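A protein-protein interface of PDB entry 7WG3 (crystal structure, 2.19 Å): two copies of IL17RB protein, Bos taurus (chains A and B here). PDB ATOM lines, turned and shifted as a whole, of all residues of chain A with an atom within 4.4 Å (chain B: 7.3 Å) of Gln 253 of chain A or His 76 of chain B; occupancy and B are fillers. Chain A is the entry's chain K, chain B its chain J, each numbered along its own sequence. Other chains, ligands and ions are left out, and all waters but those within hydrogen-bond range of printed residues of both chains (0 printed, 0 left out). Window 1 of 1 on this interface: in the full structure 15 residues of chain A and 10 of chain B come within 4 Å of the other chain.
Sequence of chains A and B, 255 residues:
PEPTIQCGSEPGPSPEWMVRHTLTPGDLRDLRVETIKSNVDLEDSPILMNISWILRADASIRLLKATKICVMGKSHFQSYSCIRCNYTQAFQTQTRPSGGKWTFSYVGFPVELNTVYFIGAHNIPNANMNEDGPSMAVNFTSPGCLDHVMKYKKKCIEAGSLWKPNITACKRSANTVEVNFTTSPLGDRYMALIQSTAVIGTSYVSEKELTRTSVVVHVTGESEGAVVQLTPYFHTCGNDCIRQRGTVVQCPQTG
No position is printed for both chains.
Of the 12 pairs that touch across the chains among the printed residues, none has its exchanged pair printed and touching as well.
Hydrophobic or aromatic side chains of chain B that line the printed part of chain A: His 76 and Phe 77.
Of the 11 printed residues of chain A, 9 touch a printed residue of chain B.
Among the printed residues, 12 pairs touch across the chains.
A ring nitrogen (NE2) of His 76 of chain B sits at hydrogen-bond distance from the side-chain amide oxygen of Gln 253 of chain A (3.3 Å).
The backbone carbonyl oxygen (O) of Ser 75 of chain B lies within hydrogen-bond range of the side-chain hydroxyl (OG1) of Thr 247 of chain A, 2.8 Å away.
O of His 76 of chain B lies within hydrogen-bond range of N of Thr 247 of chain A, 3.3 Å away.
The backbone NH (N) of Ala 169 of chain A lies within hydrogen-bond range of a ring nitrogen (ND1) of His 76 of chain B (3.2 Å).
Ile 167 of chain A touches His 76 of chain B.
O of Ile 167 of chain A touches CD1 of Phe 77 of chain B (3.6 Å).
ND1 of His 76 of chain B touches CA of Thr 168 of chain A, 3.4 Å away.
CA of Gly 246 of chain A touches O of His 76 of chain B, 3.1 Å away.
His 76 of chain B touches Val 249 of chain A.
Cys 251 of chain A touches Asp 240 of chain B (CB to OD2, 3.8 Å).
CG of Pro 252 of chain A touches OD1 of Asp 240 of chain B, at 3.5 Å.
Gln 253 of chain A touches Asn 114 of chain B (NE2 to ND2, 3.9 Å).
OG of Ser 75 of chain B lies within hydrogen-bond range of O of Asn 114 of chain B, at 3.0 Å.
The backbone NH (N) of Val 249 of chain A is in hydrogen-bond range of the backbone carbonyl oxygen (O) of Ala 169 of chain A, at 2.9 Å.
The side-chain sulfur (SG) of Cys 251 of chain A lies close to the side-chain amide oxygen (OE1) of Gln 253 of chain A (3.7 Å).
The backbone NH of Gly 144 of chain B lies close to the side-chain amide oxygen of Asn 114 of chain B (3.4 Å).
Printed residues of chain B within 4 Å of Ala 169 of chain A: His 76 (3.2 Å).
Of the printed residues of chain B, Pro 252 of chain A touches Asp 240 (3.5 Å).
Of the printed residues of chain B, Gln 253 of chain A touches His 76 (3.3 Å) and Asn 114 (3.9 Å).
Of the printed residues of chain A, Asn 114 of chain B touches Gln 253 (3.9 Å).
The nearest printed residue of chain A that does not touch His 76 of chain B is Cys 251 of chain A (4.7 Å).
The nearest printed residue of chain B that does not touch Cys 251 of chain A is His 76 of chain B (4.7 Å).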
ATOM      1  N   ILE A 167     -33.095  25.339  17.704  1.00  0.00           N
ATOM      2  CA  ILE A 167     -32.440  25.794  16.487  1.00  0.00           C
ATOM      3  C   ILE A 167     -31.043  26.288  16.823  1.00  0.00           C
ATOM      4  O   ILE A 167     -30.857  27.074  17.756  1.00  0.00           O
ATOM      5  CB  ILE A 167     -33.260  26.911  15.824  1.00  0.00           C
ATOM      6  CG1 ILE A 167     -34.645  26.412  15.405  1.00  0.00           C
ATOM      7  CG2 ILE A 167     -32.517  27.487  14.605  1.00  0.00           C
ATOM      8  CD1 ILE A 167     -35.575  27.544  14.956  1.00  0.00           C
ATOM      9  N   THR A 168     -30.047  25.784  16.109  1.00  0.00           N
ATOM     10  CA  THR A 168     -28.722  26.388  16.104  1.00  0.00           C
ATOM     11  C   THR A 168     -28.442  26.785  14.669  1.00  0.00           C
ATOM     12  O   THR A 168     -28.586  25.957  13.760  1.00  0.00           O
ATOM     13  CB  THR A 168     -27.602  25.457  16.614  1.00  0.00           C
ATOM     14  OG1 THR A 168     -27.424  24.354  15.713  1.00  0.00           O
ATOM     15  CG2 THR A 168     -27.910  24.938  18.023  1.00  0.00           C
ATOM     16  N   ALA A 169     -28.089  28.052  14.469  1.00  0.00           N
ATOM     17  CA  ALA A 169     -27.844  28.597  13.142  1.00  0.00           C
ATOM     18  C   ALA A 169     -26.544  29.388  13.151  1.00  0.00           C
ATOM     19  O   ALA A 169     -26.377  30.305  13.961  1.00  0.00           O
ATOM     20  CB  ALA A 169     -28.997  29.478  12.679  1.00  0.00           C
ATOM     21  N   GLY A 246     -35.163  31.622  15.818  1.00  0.00           N
ATOM     22  CA  GLY A 246     -33.861  31.656  16.439  1.00  0.00           C
ATOM     23  C   GLY A 246     -33.100  32.831  15.870  1.00  0.00           C
ATOM     24  O   GLY A 246     -33.699  33.683  15.214  1.00  0.00           O
ATOM     25  N   THR A 247     -31.788  32.884  16.097  1.00  0.00           N
ATOM     26  CA  THR A 247     -30.954  33.969  15.611  1.00  0.00           C
ATOM     27  C   THR A 247     -29.634  33.412  15.091  1.00  0.00           C
ATOM     28  O   THR A 247     -29.066  32.486  15.680  1.00  0.00           O
ATOM     29  CB  THR A 247     -30.718  35.007  16.721  1.00  0.00           C
ATOM     30  OG1 THR A 247     -30.154  34.355  17.859  1.00  0.00           O
ATOM     31  CG2 THR A 247     -32.034  35.708  17.133  1.00  0.00           C
ATOM     32  N   VAL A 249     -25.707  33.151  14.340  1.00  0.00           N
ATOM     33  CA  VAL A 249     -24.529  33.457  15.143  1.00  0.00           C
ATOM     34  C   VAL A 249     -23.259  33.143  14.356  1.00  0.00           C
ATOM     35  O   VAL A 249     -23.265  32.385  13.384  1.00  0.00           O
ATOM     36  CB  VAL A 249     -24.533  32.667  16.483  1.00  0.00           C
ATOM     37  CG1 VAL A 249     -23.449  33.161  17.430  1.00  0.00           C
ATOM     38  CG2 VAL A 249     -25.888  32.766  17.165  1.00  0.00           C
ATOM     39  N   GLN A 250     -22.160  33.740  14.811  1.00  0.00           N
ATOM     40  CA  GLN A 250     -20.822  33.531  14.273  1.00  0.00           C
ATOM     41  C   GLN A 250     -20.244  32.218  14.782  1.00  0.00           C
ATOM     42  O   GLN A 250     -20.051  32.065  15.990  1.00  0.00           O
ATOM     43  CB  GLN A 250     -19.921  34.685  14.710  1.00  0.00           C
ATOM     44  CG  GLN A 250     -18.485  34.635  14.209  1.00  0.00           C
ATOM     45  CD  GLN A 250     -17.641  35.762  14.793  1.00  0.00           C
ATOM     46  OE1 GLN A 250     -18.143  36.607  15.539  1.00  0.00           O
ATOM     47  NE2 GLN A 250     -16.352  35.776  14.458  1.00  0.00           N
ATOM     48  N   CYS A 251     -19.983  31.261  13.892  1.00  0.00           N
ATOM     49  CA  CYS A 251     -19.381  30.024  14.371  1.00  0.00           C
ATOM     50  C   CYS A 251     -18.047  29.791  13.672  1.00  0.00           C
ATOM     51  O   CYS A 251     -17.981  29.883  12.438  1.00  0.00           O
ATOM     52  CB  CYS A 251     -20.316  28.833  14.159  1.00  0.00           C
ATOM     53  SG  CYS A 251     -21.871  29.005  15.078  1.00  0.00           S
ATOM     54  N   PRO A 252     -16.976  29.432  14.404  1.00  0.00           N
ATOM     55  CA  PRO A 252     -16.967  28.937  15.788  1.00  0.00           C
ATOM     56  C   PRO A 252     -17.231  30.042  16.799  1.00  0.00           C
ATOM     57  O   PRO A 252     -16.981  31.218  16.526  1.00  0.00           O
ATOM     58  CB  PRO A 252     -15.536  28.419  15.967  1.00  0.00           C
ATOM     59  CG  PRO A 252     -14.983  28.306  14.590  1.00  0.00           C
ATOM     60  CD  PRO A 252     -15.628  29.401  13.820  1.00  0.00           C
ATOM     61  N   GLN A 253     -17.767  29.664  17.953  1.00  0.00           N
ATOM     62  CA  GLN A 253     -18.192  30.625  18.957  1.00  0.00           C
ATOM     63  C   GLN A 253     -17.170  30.799  20.069  1.00  0.00           C
ATOM     64  O   GLN A 253     -17.317  31.714  20.888  1.00  0.00           O
ATOM     65  CB  GLN A 253     -19.538  30.191  19.542  1.00  0.00           C
ATOM     66  CG  GLN A 253     -20.480  29.646  18.482  1.00  0.00           C
ATOM     67  CD  GLN A 253     -21.785  29.147  19.052  1.00  0.00           C
ATOM     68  OE1 GLN A 253     -22.295  28.101  18.642  1.00  0.00           O
ATOM     69  NE2 GLN A 253     -22.344  29.899  19.994  1.00  0.00           N
ATOM     70  N   THR A 254     -16.138  29.961  20.088  1.00  0.00           N
ATOM     71  CA  THR A 254     -15.091  29.948  21.095  1.00  0.00           C
ATOM     72  C   THR A 254     -13.811  30.558  20.532  1.00  0.00           C
ATOM     73  O   THR A 254     -13.678  30.793  19.327  1.00  0.00           O
ATOM     74  CB  THR A 254     -14.823  28.511  21.560  1.00  0.00           C
ATOM     75  OG1 THR A 254     -13.921  27.881  20.637  1.00  0.00           O
ATOM     76  CG2 THR A 254     -16.123  27.710  21.589  1.00  0.00           C
ATOM     77  N   GLY B  73     -33.746  33.597  28.383  1.00  0.00           N
ATOM     78  CA  GLY B  73     -32.457  33.341  27.760  1.00  0.00           C
ATOM     79  C   GLY B  73     -32.508  33.608  26.266  1.00  0.00           C
ATOM     80  O   GLY B  73     -33.399  33.119  25.569  1.00  0.00           O
ATOM     81  N   LYS B  74     -31.526  34.358  25.777  1.00  0.00           N
ATOM     82  CA  LYS B  74     -31.405  34.624  24.346  1.00  0.00           C
ATOM     83  C   LYS B  74     -30.012  34.197  23.886  1.00  0.00           C
ATOM     84  O   LYS B  74     -29.002  34.792  24.276  1.00  0.00           O
ATOM     85  CB  LYS B  74     -31.694  36.097  24.052  1.00  0.00           C
ATOM     86  CG  LYS B  74     -33.140  36.505  24.382  1.00  0.00           C
ATOM     87  CD  LYS B  74     -33.742  37.637  23.528  1.00  0.00           C
ATOM     88  CE  LYS B  74     -32.739  38.680  23.002  1.00  0.00           C
ATOM     89  NZ  LYS B  74     -31.806  38.225  21.918  1.00  0.00           N
ATOM     90  N   SER B  75     -29.953  33.136  23.095  1.00  0.00           N
ATOM     91  CA  SER B  75     -28.695  32.698  22.508  1.00  0.00           C
ATOM     92  C   SER B  75     -28.954  32.359  21.055  1.00  0.00           C
ATOM     93  O   SER B  75     -29.052  33.249  20.207  1.00  0.00           O
ATOM     94  CB  SER B  75     -28.122  31.484  23.250  1.00  0.00           C
ATOM     95  OG  SER B  75     -27.031  30.903  22.542  1.00  0.00           O
ATOM     96  N   HIS B  76     -29.082  31.066  20.772  1.00  0.00           N
ATOM     97  CA  HIS B  76     -29.561  30.612  19.478  1.00  0.00           C
ATOM     98  C   HIS B  76     -31.078  30.630  19.379  1.00  0.00           C
ATOM     99  O   HIS B  76     -31.602  30.458  18.276  1.00  0.00           O
ATOM    100  CB  HIS B  76     -29.047  29.201  19.197  1.00  0.00           C
ATOM    101  CG  HIS B  76     -27.642  29.162  18.686  1.00  0.00           C
ATOM    102  ND1 HIS B  76     -27.337  29.247  17.340  1.00  0.00           N
ATOM    103  CD2 HIS B  76     -26.460  29.038  19.334  1.00  0.00           C
ATOM    104  CE1 HIS B  76     -26.025  29.176  17.187  1.00  0.00           C
ATOM    105  NE2 HIS B  76     -25.471  29.048  18.380  1.00  0.00           N
ATOM    106  N   PHE B  77     -31.779  30.819  20.498  1.00  0.00           N
ATOM    107  CA  PHE B  77     -33.234  30.922  20.564  1.00  0.00           C
ATOM    108  C   PHE B  77     -33.618  31.360  21.970  1.00  0.00           C
ATOM    109  O   PHE B  77     -32.827  31.247  22.911  1.00  0.00           O
ATOM    110  CB  PHE B  77     -33.927  29.598  20.224  1.00  0.00           C
ATOM    111  CG  PHE B  77     -33.557  28.481  21.148  1.00  0.00           C
ATOM    112  CD1 PHE B  77     -32.422  27.728  20.911  1.00  0.00           C
ATOM    113  CD2 PHE B  77     -34.339  28.190  22.265  1.00  0.00           C
ATOM    114  CE1 PHE B  77     -32.073  26.712  21.767  1.00  0.00           C
ATOM    115  CE2 PHE B  77     -33.994  27.164  23.124  1.00  0.00           C
ATOM    116  CZ  PHE B  77     -32.863  26.419  22.872  1.00  0.00           C
ATOM    117  N   GLN B  78     -34.849  31.840  22.099  1.00  0.00           N
ATOM    118  CA  GLN B  78     -35.350  32.303  23.382  1.00  0.00           C
ATOM    119  C   GLN B  78     -35.887  31.155  24.229  1.00  0.00           C
ATOM    120  O   GLN B  78     -36.422  30.166  23.716  1.00  0.00           O
ATOM    121  CB  GLN B  78     -36.461  33.328  23.195  1.00  0.00           C
ATOM    122  CG  GLN B  78     -36.008  34.691  22.752  1.00  0.00           C
ATOM    123  CD  GLN B  78     -37.166  35.655  22.747  1.00  0.00           C
ATOM    124  OE1 GLN B  78     -38.253  35.317  23.219  1.00  0.00           O
ATOM    125  NE2 GLN B  78     -36.952  36.855  22.215  1.00  0.00           N
ATOM    126  N   GLU B 112     -27.332  27.675  30.277  1.00  0.00           N
ATOM    127  CA  GLU B 112     -26.747  27.161  29.051  1.00  0.00           C
ATOM    128  C   GLU B 112     -25.537  28.004  28.650  1.00  0.00           C
ATOM    129  O   GLU B 112     -25.333  29.119  29.138  1.00  0.00           O
ATOM    130  CB  GLU B 112     -27.795  27.135  27.938  1.00  0.00           C
ATOM    131  CG  GLU B 112     -28.949  26.181  28.215  1.00  0.00           C
ATOM    132  CD  GLU B 112     -29.972  26.105  27.070  1.00  0.00           C
ATOM    133  OE1 GLU B 112     -29.799  26.815  26.050  1.00  0.00           O
ATOM    134  OE2 GLU B 112     -30.959  25.339  27.193  1.00  0.00           O
ATOM    135  N   LEU B 113     -24.712  27.444  27.772  1.00  0.00           N
ATOM    136  CA  LEU B 113     -23.526  28.148  27.310  1.00  0.00           C
ATOM    137  C   LEU B 113     -23.898  29.328  26.416  1.00  0.00           C
ATOM    138  O   LEU B 113     -24.901  29.301  25.704  1.00  0.00           O
ATOM    139  CB  LEU B 113     -22.606  27.193  26.541  1.00  0.00           C
ATOM    140  CG  LEU B 113     -21.849  26.117  27.322  1.00  0.00           C
ATOM    141  CD1 LEU B 113     -21.719  24.867  26.455  1.00  0.00           C
ATOM    142  CD2 LEU B 113     -20.483  26.571  27.833  1.00  0.00           C
ATOM    143  N   ASN B 114     -23.073  30.374  26.469  1.00  0.00           N
ATOM    144  CA  ASN B 114     -23.101  31.477  25.501  1.00  0.00           C
ATOM    145  C   ASN B 114     -24.495  32.072  25.330  1.00  0.00           C
ATOM    146  O   ASN B 114     -24.950  32.321  24.211  1.00  0.00           O
ATOM    147  CB  ASN B 114     -22.592  31.004  24.136  1.00  0.00           C
ATOM    148  CG  ASN B 114     -21.142  30.608  24.156  1.00  0.00           C
ATOM    149  OD1 ASN B 114     -20.293  31.307  24.698  1.00  0.00           O
ATOM    150  ND2 ASN B 114     -20.854  29.444  23.585  1.00  0.00           N
ATOM    151  N   THR B 115     -25.181  32.313  26.442  1.00  0.00           N
ATOM    152  CA  THR B 115     -26.540  32.844  26.389  1.00  0.00           C
ATOM    153  C   THR B 115     -26.611  34.146  27.166  1.00  0.00           C
ATOM    154  O   THR B 115     -25.965  34.294  28.210  1.00  0.00           O
ATOM    155  CB  THR B 115     -27.576  31.855  26.959  1.00  0.00           C
ATOM    156  OG1 THR B 115     -27.548  30.632  26.215  1.00  0.00           O
ATOM    157  CG2 THR B 115     -28.983  32.440  26.893  1.00  0.00           C
ATOM    158  N   GLY B 144     -18.638  30.763  27.663  1.00  0.00           N
ATOM    159  CA  GLY B 144     -18.528  29.615  26.811  1.00  0.00           C
ATOM    160  C   GLY B 144     -17.550  28.592  27.345  1.00  0.00           C
ATOM    161  O   GLY B 144     -17.204  28.570  28.535  1.00  0.00           O
ATOM    162  N   CYS B 145     -17.089  27.728  26.447  1.00  0.00           N
ATOM    163  CA  CYS B 145     -16.296  26.574  26.835  1.00  0.00           C
ATOM    164  C   CYS B 145     -14.898  26.933  27.312  1.00  0.00           C
ATOM    165  O   CYS B 145     -14.189  26.048  27.797  1.00  0.00           O
ATOM    166  CB  CYS B 145     -16.229  25.611  25.658  1.00  0.00           C
ATOM    167  SG  CYS B 145     -17.770  24.774  25.392  1.00  0.00           S
ATOM    168  N   LEU B 146     -14.481  28.193  27.187  1.00  0.00           N
ATOM    169  CA  LEU B 146     -13.199  28.634  27.724  1.00  0.00           C
ATOM    170  C   LEU B 146     -13.299  29.101  29.171  1.00  0.00           C
ATOM    171  O   LEU B 146     -12.267  29.324  29.812  1.00  0.00           O
ATOM    172  CB  LEU B 146     -12.591  29.734  26.841  1.00  0.00           C
ATOM    173  CG  LEU B 146     -12.306  29.304  25.399  1.00  0.00           C
ATOM    174  CD1 LEU B 146     -11.788  30.459  24.587  1.00  0.00           C
ATOM    175  CD2 LEU B 146     -11.293  28.185  25.393  1.00  0.00           C
ATOM    176  N   ASP B 240     -16.270  23.210  14.358  1.00  0.00           N
ATOM    177  CA  ASP B 240     -16.289  24.262  15.369  1.00  0.00           C
ATOM    178  C   ASP B 240     -15.774  23.792  16.737  1.00  0.00           C
ATOM    179  O   ASP B 240     -16.242  24.273  17.774  1.00  0.00           O
ATOM    180  CB  ASP B 240     -17.694  24.848  15.468  1.00  0.00           C
ATOM    181  CG  ASP B 240     -18.171  25.436  14.137  1.00  0.00           C
ATOM    182  OD1 ASP B 240     -17.352  26.075  13.417  1.00  0.00           O
ATOM    183  OD2 ASP B 240     -19.354  25.212  13.791  1.00  0.00           O
ATOM    184  N   ARG B 243     -10.049  25.411  19.214  1.00  0.00           N
ATOM    185  CA  ARG B 243      -8.701  25.421  18.647  1.00  0.00           C
ATOM    186  C   ARG B 243      -7.639  25.802  19.662  1.00  0.00           C
ATOM    187  O   ARG B 243      -7.894  26.531  20.620  1.00  0.00           O
ATOM    188  CB  ARG B 243      -8.583  26.335  17.425  1.00  0.00           C
ATOM    189  CG  ARG B 243      -9.026  25.651  16.183  1.00  0.00           C
ATOM    190  CD  ARG B 243     -10.475  25.526  16.166  1.00  0.00           C
ATOM    191  NE  ARG B 243     -10.943  24.782  14.994  1.00  0.00           N
ATOM    192  CZ  ARG B 243     -12.217  24.476  14.818  1.00  0.00           C
ATOM    193  NH1 ARG B 243     -13.135  24.818  15.703  1.00  0.00           N
ATOM    194  NH2 ARG B 243     -12.582  23.845  13.728  1.00  0.00           N
